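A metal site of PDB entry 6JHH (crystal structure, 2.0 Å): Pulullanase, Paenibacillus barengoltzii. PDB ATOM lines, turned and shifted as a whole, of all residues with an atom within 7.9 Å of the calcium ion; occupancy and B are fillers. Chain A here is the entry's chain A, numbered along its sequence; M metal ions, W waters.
The calcium ion is bound by water W2 (2.3 Å), the side-chain carboxylate (OE2) of Glu 224 (2.3 Å), the side-chain carboxylate (OD1) of Asp 216 (2.3 Å), water W1 (2.4 Å), the backbone carbonyl oxygen (O) of Tyr 217 (2.4 Å) and the side-chain carboxylate (OE1) of Glu 245 (2.5 Å).
Four residues have an atom within 4 Å of the calcium ion: Asp 216, Tyr 217, Glu 224 and Glu 245.
Water W1 lies within hydrogen-bond range of the side-chain carboxylate of Glu 245 and the backbone carbonyl oxygen of Val 222.
Water W2 bridges OE1 of Gln 239 and O of Asn 125.
The side-chain carboxylate of Glu 224 lies close to the backbone NH of Gly 246, 3.1 Å away.
The side-chain carboxylate of Glu 224 lies within hydrogen-bond range of the backbone NH of Asn 125, at 2.7 Å.
O of Asp 216 sits at hydrogen-bond distance from N of Gln 239 (2.9 Å).
NH1 of Arg 258 sits close to OD1 of Asp 216 (3.96 Å).
The side-chain amide nitrogen of Asn 240 sits at hydrogen-bond distance from the side-chain carboxylate of Asp 216 (3.0 Å).
The backbone NH (N) of Asp 216 sits at hydrogen-bond distance from the backbone carbonyl oxygen (O) of Val 243 (2.8 Å).
The side-chain hydroxyl of Tyr 217 sits at hydrogen-bond distance from the side-chain hydroxyl of Tyr 248 (2.8 Å).
OE2 of Glu 245 sits at hydrogen-bond distance from OG of Ser 247 (2.4 Å).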
ATOM      1  N   VAL A 122      18.326   3.310 -26.920  1.00  0.00           N
ATOM      2  CA  VAL A 122      18.100   3.502 -25.488  1.00  0.00           C
ATOM      3  C   VAL A 122      18.033   2.149 -24.808  1.00  0.00           C
ATOM      4  O   VAL A 122      17.804   1.114 -25.432  1.00  0.00           O
ATOM      5  CB  VAL A 122      16.794   4.273 -25.176  1.00  0.00           C
ATOM      6  CG1 VAL A 122      16.860   5.724 -25.658  1.00  0.00           C
ATOM      7  CG2 VAL A 122      15.602   3.522 -25.747  1.00  0.00           C
ATOM      8  N   GLY A 123      18.208   2.168 -23.475  1.00  0.00           N
ATOM      9  CA  GLY A 123      17.894   1.020 -22.657  1.00  0.00           C
ATOM     10  C   GLY A 123      16.393   0.938 -22.389  1.00  0.00           C
ATOM     11  O   GLY A 123      15.589   1.723 -22.891  1.00  0.00           O
ATOM     12  N   VAL A 124      16.024  -0.062 -21.574  1.00  0.00           N
ATOM     13  CA  VAL A 124      14.618  -0.344 -21.330  1.00  0.00           C
ATOM     14  C   VAL A 124      13.939   0.897 -20.769  1.00  0.00           C
ATOM     15  O   VAL A 124      14.486   1.609 -19.920  1.00  0.00           O
ATOM     16  CB  VAL A 124      14.460  -1.558 -20.388  1.00  0.00           C
ATOM     17  CG1 VAL A 124      15.281  -1.379 -19.111  1.00  0.00           C
ATOM     18  CG2 VAL A 124      12.982  -1.814 -20.051  1.00  0.00           C
ATOM     19  N   ASN A 125      12.742   1.183 -21.289  1.00  0.00           N
ATOM     20  CA  ASN A 125      11.897   2.314 -20.882  1.00  0.00           C
ATOM     21  C   ASN A 125      12.527   3.664 -21.174  1.00  0.00           C
ATOM     22  O   ASN A 125      12.045   4.686 -20.673  1.00  0.00           O
ATOM     23  CB  ASN A 125      11.496   2.220 -19.397  1.00  0.00           C
ATOM     24  CG  ASN A 125      10.303   1.297 -19.177  1.00  0.00           C
ATOM     25  OD1 ASN A 125       9.434   1.186 -20.043  1.00  0.00           O
ATOM     26  ND2 ASN A 125      10.268   0.620 -18.030  1.00  0.00           N
ATOM     27  N   GLY A 126      13.609   3.700 -21.943  1.00  0.00           N
ATOM     28  CA  GLY A 126      14.060   4.949 -22.549  1.00  0.00           C
ATOM     29  C   GLY A 126      14.637   6.010 -21.637  1.00  0.00           C
ATOM     30  O   GLY A 126      14.492   7.197 -21.932  1.00  0.00           O
ATOM     31  N   TYR A 215       7.592   4.766 -32.830  1.00  0.00           N
ATOM     32  CA  TYR A 215       8.595   5.435 -32.017  1.00  0.00           C
ATOM     33  C   TYR A 215       8.394   5.036 -30.550  1.00  0.00           C
ATOM     34  O   TYR A 215       7.379   4.434 -30.167  1.00  0.00           O
ATOM     35  CB  TYR A 215       8.496   6.956 -32.196  1.00  0.00           C
ATOM     36  CG  TYR A 215       7.125   7.453 -31.822  1.00  0.00           C
ATOM     37  CD1 TYR A 215       6.788   7.650 -30.485  1.00  0.00           C
ATOM     38  CD2 TYR A 215       6.169   7.692 -32.781  1.00  0.00           C
ATOM     39  CE1 TYR A 215       5.531   8.080 -30.113  1.00  0.00           C
ATOM     40  CE2 TYR A 215       4.894   8.139 -32.414  1.00  0.00           C
ATOM     41  CZ  TYR A 215       4.596   8.326 -31.068  1.00  0.00           C
ATOM     42  OH  TYR A 215       3.330   8.745 -30.680  1.00  0.00           O
ATOM     43  N   ASP A 216       9.338   5.447 -29.709  1.00  0.00           N
ATOM     44  CA  ASP A 216       9.345   5.044 -28.310  1.00  0.00           C
ATOM     45  C   ASP A 216       8.375   5.920 -27.516  1.00  0.00           C
ATOM     46  O   ASP A 216       8.642   7.110 -27.285  1.00  0.00           O
ATOM     47  CB  ASP A 216      10.762   5.148 -27.767  1.00  0.00           C
ATOM     48  CG  ASP A 216      10.898   4.559 -26.363  1.00  0.00           C
ATOM     49  OD1 ASP A 216      10.072   3.699 -26.007  1.00  0.00           O
ATOM     50  OD2 ASP A 216      11.819   4.954 -25.644  1.00  0.00           O
ATOM     51  N   TYR A 217       7.261   5.346 -27.077  1.00  0.00           N
ATOM     52  CA  TYR A 217       6.299   6.112 -26.309  1.00  0.00           C
ATOM     53  C   TYR A 217       6.452   5.798 -24.812  1.00  0.00           C
ATOM     54  O   TYR A 217       7.269   4.977 -24.420  1.00  0.00           O
ATOM     55  CB  TYR A 217       4.881   5.873 -26.842  1.00  0.00           C
ATOM     56  CG  TYR A 217       4.401   4.449 -26.967  1.00  0.00           C
ATOM     57  CD1 TYR A 217       3.896   3.771 -25.861  1.00  0.00           C
ATOM     58  CD2 TYR A 217       4.366   3.815 -28.206  1.00  0.00           C
ATOM     59  CE1 TYR A 217       3.399   2.485 -25.981  1.00  0.00           C
ATOM     60  CE2 TYR A 217       3.881   2.522 -28.330  1.00  0.00           C
ATOM     61  CZ  TYR A 217       3.398   1.864 -27.216  1.00  0.00           C
ATOM     62  OH  TYR A 217       2.907   0.595 -27.344  1.00  0.00           O
ATOM     63  N   SER A 218       5.663   6.467 -23.968  1.00  0.00           N
ATOM     64  CA  SER A 218       6.064   6.605 -22.563  1.00  0.00           C
ATOM     65  C   SER A 218       5.844   5.316 -21.770  1.00  0.00           C
ATOM     66  O   SER A 218       5.014   4.459 -22.100  1.00  0.00           O
ATOM     67  CB  SER A 218       5.302   7.738 -21.877  1.00  0.00           C
ATOM     68  OG  SER A 218       4.002   7.321 -21.496  1.00  0.00           O
ATOM     69  N   GLN A 219       6.607   5.206 -20.668  1.00  0.00           N
ATOM     70  CA  GLN A 219       6.501   4.085 -19.739  1.00  0.00           C
ATOM     71  C   GLN A 219       5.133   4.003 -19.062  1.00  0.00           C
ATOM     72  O   GLN A 219       4.649   2.903 -18.772  1.00  0.00           O
ATOM     73  CB  GLN A 219       7.619   4.194 -18.692  1.00  0.00           C
ATOM     74  CG  GLN A 219       7.392   3.357 -17.441  1.00  0.00           C
ATOM     75  CD  GLN A 219       8.627   3.243 -16.569  1.00  0.00           C
ATOM     76  OE1 GLN A 219       9.680   3.796 -16.881  1.00  0.00           O
ATOM     77  NE2 GLN A 219       8.499   2.503 -15.455  1.00  0.00           N
ATOM     78  N   GLU A 220       4.488   5.144 -18.821  1.00  0.00           N
ATOM     79  CA  GLU A 220       3.175   5.121 -18.197  1.00  0.00           C
ATOM     80  C   GLU A 220       2.115   4.518 -19.109  1.00  0.00           C
ATOM     81  O   GLU A 220       1.059   4.108 -18.627  1.00  0.00           O
ATOM     82  CB  GLU A 220       2.733   6.529 -17.788  1.00  0.00           C
ATOM     83  CG  GLU A 220       3.632   7.208 -16.748  1.00  0.00           C
ATOM     84  CD  GLU A 220       5.013   7.543 -17.282  1.00  0.00           C
ATOM     85  OE1 GLU A 220       5.984   7.538 -16.504  1.00  0.00           O
ATOM     86  OE2 GLU A 220       5.127   7.800 -18.507  1.00  0.00           O
ATOM     87  N   SER A 221       2.372   4.468 -20.421  1.00  0.00           N
ATOM     88  CA  SER A 221       1.413   3.891 -21.349  1.00  0.00           C
ATOM     89  C   SER A 221       1.607   2.388 -21.444  1.00  0.00           C
ATOM     90  O   SER A 221       0.648   1.625 -21.298  1.00  0.00           O
ATOM     91  CB  SER A 221       1.551   4.531 -22.731  1.00  0.00           C
ATOM     92  OG  SER A 221       1.473   5.935 -22.629  1.00  0.00           O
ATOM     93  N   VAL A 222       2.845   1.949 -21.680  1.00  0.00           N
ATOM     94  CA  VAL A 222       3.220   0.545 -21.608  1.00  0.00           C
ATOM     95  C   VAL A 222       4.568   0.476 -20.895  1.00  0.00           C
ATOM     96  O   VAL A 222       5.556   1.026 -21.379  1.00  0.00           O
ATOM     97  CB  VAL A 222       3.325  -0.130 -22.992  1.00  0.00           C
ATOM     98  CG1 VAL A 222       3.765  -1.560 -22.829  1.00  0.00           C
ATOM     99  CG2 VAL A 222       1.961  -0.077 -23.725  1.00  0.00           C
ATOM    100  N   ASP A 223       4.612  -0.222 -19.755  1.00  0.00           N
ATOM    101  CA  ASP A 223       5.862  -0.389 -19.029  1.00  0.00           C
ATOM    102  C   ASP A 223       6.642  -1.551 -19.640  1.00  0.00           C
ATOM    103  O   ASP A 223       6.250  -2.708 -19.516  1.00  0.00           O
ATOM    104  CB  ASP A 223       5.591  -0.629 -17.553  1.00  0.00           C
ATOM    105  CG  ASP A 223       6.854  -0.571 -16.716  1.00  0.00           C
ATOM    106  OD1 ASP A 223       7.963  -0.852 -17.250  1.00  0.00           O
ATOM    107  OD2 ASP A 223       6.736  -0.232 -15.522  1.00  0.00           O
ATOM    108  N   GLU A 224       7.798  -1.239 -20.245  1.00  0.00           N
ATOM    109  CA  GLU A 224       8.601  -2.247 -20.932  1.00  0.00           C
ATOM    110  C   GLU A 224       9.271  -3.245 -19.987  1.00  0.00           C
ATOM    111  O   GLU A 224       9.858  -4.223 -20.464  1.00  0.00           O
ATOM    112  CB  GLU A 224       9.688  -1.563 -21.786  1.00  0.00           C
ATOM    113  CG  GLU A 224       9.142  -0.704 -22.944  1.00  0.00           C
ATOM    114  CD  GLU A 224      10.209   0.167 -23.601  1.00  0.00           C
ATOM    115  OE1 GLU A 224      11.415  -0.066 -23.347  1.00  0.00           O
ATOM    116  OE2 GLU A 224       9.854   1.082 -24.362  1.00  0.00           O
ATOM    117  N   ASP A 237       1.890   9.044 -26.955  1.00  0.00           N
ATOM    118  CA  ASP A 237       2.571   9.701 -25.835  1.00  0.00           C
ATOM    119  C   ASP A 237       4.080   9.647 -26.088  1.00  0.00           C
ATOM    120  O   ASP A 237       4.794   8.808 -25.526  1.00  0.00           O
ATOM    121  CB  ASP A 237       2.201   9.022 -24.515  1.00  0.00           C
ATOM    122  CG  ASP A 237       0.687   8.740 -24.399  1.00  0.00           C
ATOM    123  OD1 ASP A 237      -0.120   9.710 -24.385  1.00  0.00           O
ATOM    124  OD2 ASP A 237       0.298   7.550 -24.315  1.00  0.00           O
ATOM    125  N   GLN A 239       8.005   9.736 -26.192  1.00  0.00           N
ATOM    126  CA  GLN A 239       9.111   9.823 -25.247  1.00  0.00           C
ATOM    127  C   GLN A 239      10.439  10.054 -25.960  1.00  0.00           C
ATOM    128  O   GLN A 239      11.093  11.080 -25.728  1.00  0.00           O
ATOM    129  CB  GLN A 239       9.192   8.556 -24.379  1.00  0.00           C
ATOM    130  CG  GLN A 239       9.569   8.829 -22.907  1.00  0.00           C
ATOM    131  CD  GLN A 239      10.130   7.598 -22.203  1.00  0.00           C
ATOM    132  OE1 GLN A 239       9.428   6.628 -21.930  1.00  0.00           O
ATOM    133  NE2 GLN A 239      11.428   7.637 -21.925  1.00  0.00           N
ATOM    134  N   ASN A 240      10.869   9.142 -26.823  1.00  0.00           N
ATOM    135  CA  ASN A 240      12.062   9.337 -27.638  1.00  0.00           C
ATOM    136  C   ASN A 240      11.692   9.258 -29.118  1.00  0.00           C
ATOM    137  O   ASN A 240      11.389   8.168 -29.623  1.00  0.00           O
ATOM    138  CB  ASN A 240      13.131   8.317 -27.274  1.00  0.00           C
ATOM    139  CG  ASN A 240      13.586   8.461 -25.840  1.00  0.00           C
ATOM    140  OD1 ASN A 240      14.191   9.473 -25.457  1.00  0.00           O
ATOM    141  ND2 ASN A 240      13.298   7.449 -25.012  1.00  0.00           N
ATOM    142  N   VAL A 243      13.846   6.652 -31.874  1.00  0.00           N
ATOM    143  CA  VAL A 243      14.123   5.235 -31.570  1.00  0.00           C
ATOM    144  C   VAL A 243      12.811   4.481 -31.452  1.00  0.00           C
ATOM    145  O   VAL A 243      11.766   5.039 -31.093  1.00  0.00           O
ATOM    146  CB  VAL A 243      14.950   5.115 -30.251  1.00  0.00           C
ATOM    147  CG1 VAL A 243      14.186   5.637 -29.094  1.00  0.00           C
ATOM    148  CG2 VAL A 243      15.402   3.694 -29.966  1.00  0.00           C
ATOM    149  N   PRO A 244      12.822   3.186 -31.809  1.00  0.00           N
ATOM    150  CA  PRO A 244      11.576   2.390 -31.751  1.00  0.00           C
ATOM    151  C   PRO A 244      11.075   2.146 -30.333  1.00  0.00           C
ATOM    152  O   PRO A 244      11.789   2.227 -29.333  1.00  0.00           O
ATOM    153  CB  PRO A 244      11.966   1.067 -32.407  1.00  0.00           C
ATOM    154  CG  PRO A 244      13.130   1.378 -33.270  1.00  0.00           C
ATOM    155  CD  PRO A 244      13.880   2.479 -32.552  1.00  0.00           C
ATOM    156  N   GLU A 245       9.788   1.790 -30.271  1.00  0.00           N
ATOM    157  CA  GLU A 245       9.128   1.413 -29.028  1.00  0.00           C
ATOM    158  C   GLU A 245       9.651   0.067 -28.540  1.00  0.00           C
ATOM    159  O   GLU A 245       9.722  -0.891 -29.310  1.00  0.00           O
ATOM    160  CB  GLU A 245       7.609   1.384 -29.235  1.00  0.00           C
ATOM    161  CG  GLU A 245       6.824   0.500 -28.278  1.00  0.00           C
ATOM    162  CD  GLU A 245       6.949   0.971 -26.827  1.00  0.00           C
ATOM    163  OE1 GLU A 245       7.345   2.124 -26.624  1.00  0.00           O
ATOM    164  OE2 GLU A 245       6.623   0.189 -25.897  1.00  0.00           O
ATOM    165  N   GLY A 246      10.000   0.002 -27.250  1.00  0.00           N
ATOM    166  CA  GLY A 246      10.623  -1.209 -26.722  1.00  0.00           C
ATOM    167  C   GLY A 246       9.697  -2.398 -26.630  1.00  0.00           C
ATOM    168  O   GLY A 246      10.130  -3.543 -26.799  1.00  0.00           O
ATOM    169  N   SER A 247       8.406  -2.159 -26.362  1.00  0.00           N
ATOM    170  CA  SER A 247       7.509  -3.287 -26.124  1.00  0.00           C
ATOM    171  C   SER A 247       7.199  -4.067 -27.387  1.00  0.00           C
ATOM    172  O   SER A 247       6.681  -5.179 -27.265  1.00  0.00           O
ATOM    173  CB  SER A 247       6.205  -2.817 -25.472  1.00  0.00           C
ATOM    174  OG  SER A 247       5.492  -1.910 -26.302  1.00  0.00           O
ATOM    175  N   TYR A 248       7.516  -3.544 -28.566  1.00  0.00           N
ATOM    176  CA  TYR A 248       7.339  -4.298 -29.795  1.00  0.00           C
ATOM    177  C   TYR A 248       8.556  -5.143 -30.155  1.00  0.00           C
ATOM    178  O   TYR A 248       8.510  -5.867 -31.156  1.00  0.00           O
ATOM    179  CB  TYR A 248       6.984  -3.344 -30.953  1.00  0.00           C
ATOM    180  CG  TYR A 248       5.730  -2.536 -30.695  1.00  0.00           C
ATOM    181  CD1 TYR A 248       4.687  -3.060 -29.938  1.00  0.00           C
ATOM    182  CD2 TYR A 248       5.590  -1.236 -31.184  1.00  0.00           C
ATOM    183  CE1 TYR A 248       3.541  -2.322 -29.669  1.00  0.00           C
ATOM    184  CE2 TYR A 248       4.445  -0.498 -30.940  1.00  0.00           C
ATOM    185  CZ  TYR A 248       3.422  -1.044 -30.186  1.00  0.00           C
ATOM    186  OH  TYR A 248       2.283  -0.315 -29.934  1.00  0.00           O
ATOM    187  N   PRO A 252      13.316  -5.686 -24.816  1.00  0.00           N
ATOM    188  CA  PRO A 252      13.480  -4.229 -24.644  1.00  0.00           C
ATOM    189  C   PRO A 252      14.710  -3.855 -23.833  1.00  0.00           C
ATOM    190  O   PRO A 252      15.093  -2.682 -23.859  1.00  0.00           O
ATOM    191  CB  PRO A 252      12.187  -3.806 -23.934  1.00  0.00           C
ATOM    192  CG  PRO A 252      11.604  -5.055 -23.377  1.00  0.00           C
ATOM    193  CD  PRO A 252      12.108  -6.212 -24.182  1.00  0.00           C
ATOM    194  N   ARG A 258      15.403  -3.919 -30.768  1.00  0.00           N
ATOM    195  CA  ARG A 258      14.218  -3.298 -31.359  1.00  0.00           C
ATOM    196  C   ARG A 258      14.546  -2.644 -32.691  1.00  0.00           C
ATOM    197  O   ARG A 258      13.682  -2.543 -33.577  1.00  0.00           O
ATOM    198  CB  ARG A 258      13.642  -2.268 -30.389  1.00  0.00           C
ATOM    199  CG  ARG A 258      14.629  -1.122 -30.096  1.00  0.00           C
ATOM    200  CD  ARG A 258      14.113  -0.095 -29.064  1.00  0.00           C
ATOM    201  NE  ARG A 258      14.250  -0.549 -27.671  1.00  0.00           N
ATOM    202  CZ  ARG A 258      13.732   0.099 -26.624  1.00  0.00           C
ATOM    203  NH1 ARG A 258      13.060   1.227 -26.832  1.00  0.00           N
ATOM    204  NH2 ARG A 258      13.861  -0.383 -25.390  1.00  0.00           N
HETATM  205 CA    CA M   1       8.436   2.914 -24.551  1.00  0.00          CA
HETATM  206  O   HOH W   1       6.472   1.794 -23.852  1.00  0.00           O
HETATM  207  O   HOH W   2       9.464   3.521 -22.635  1.00  0.00           O
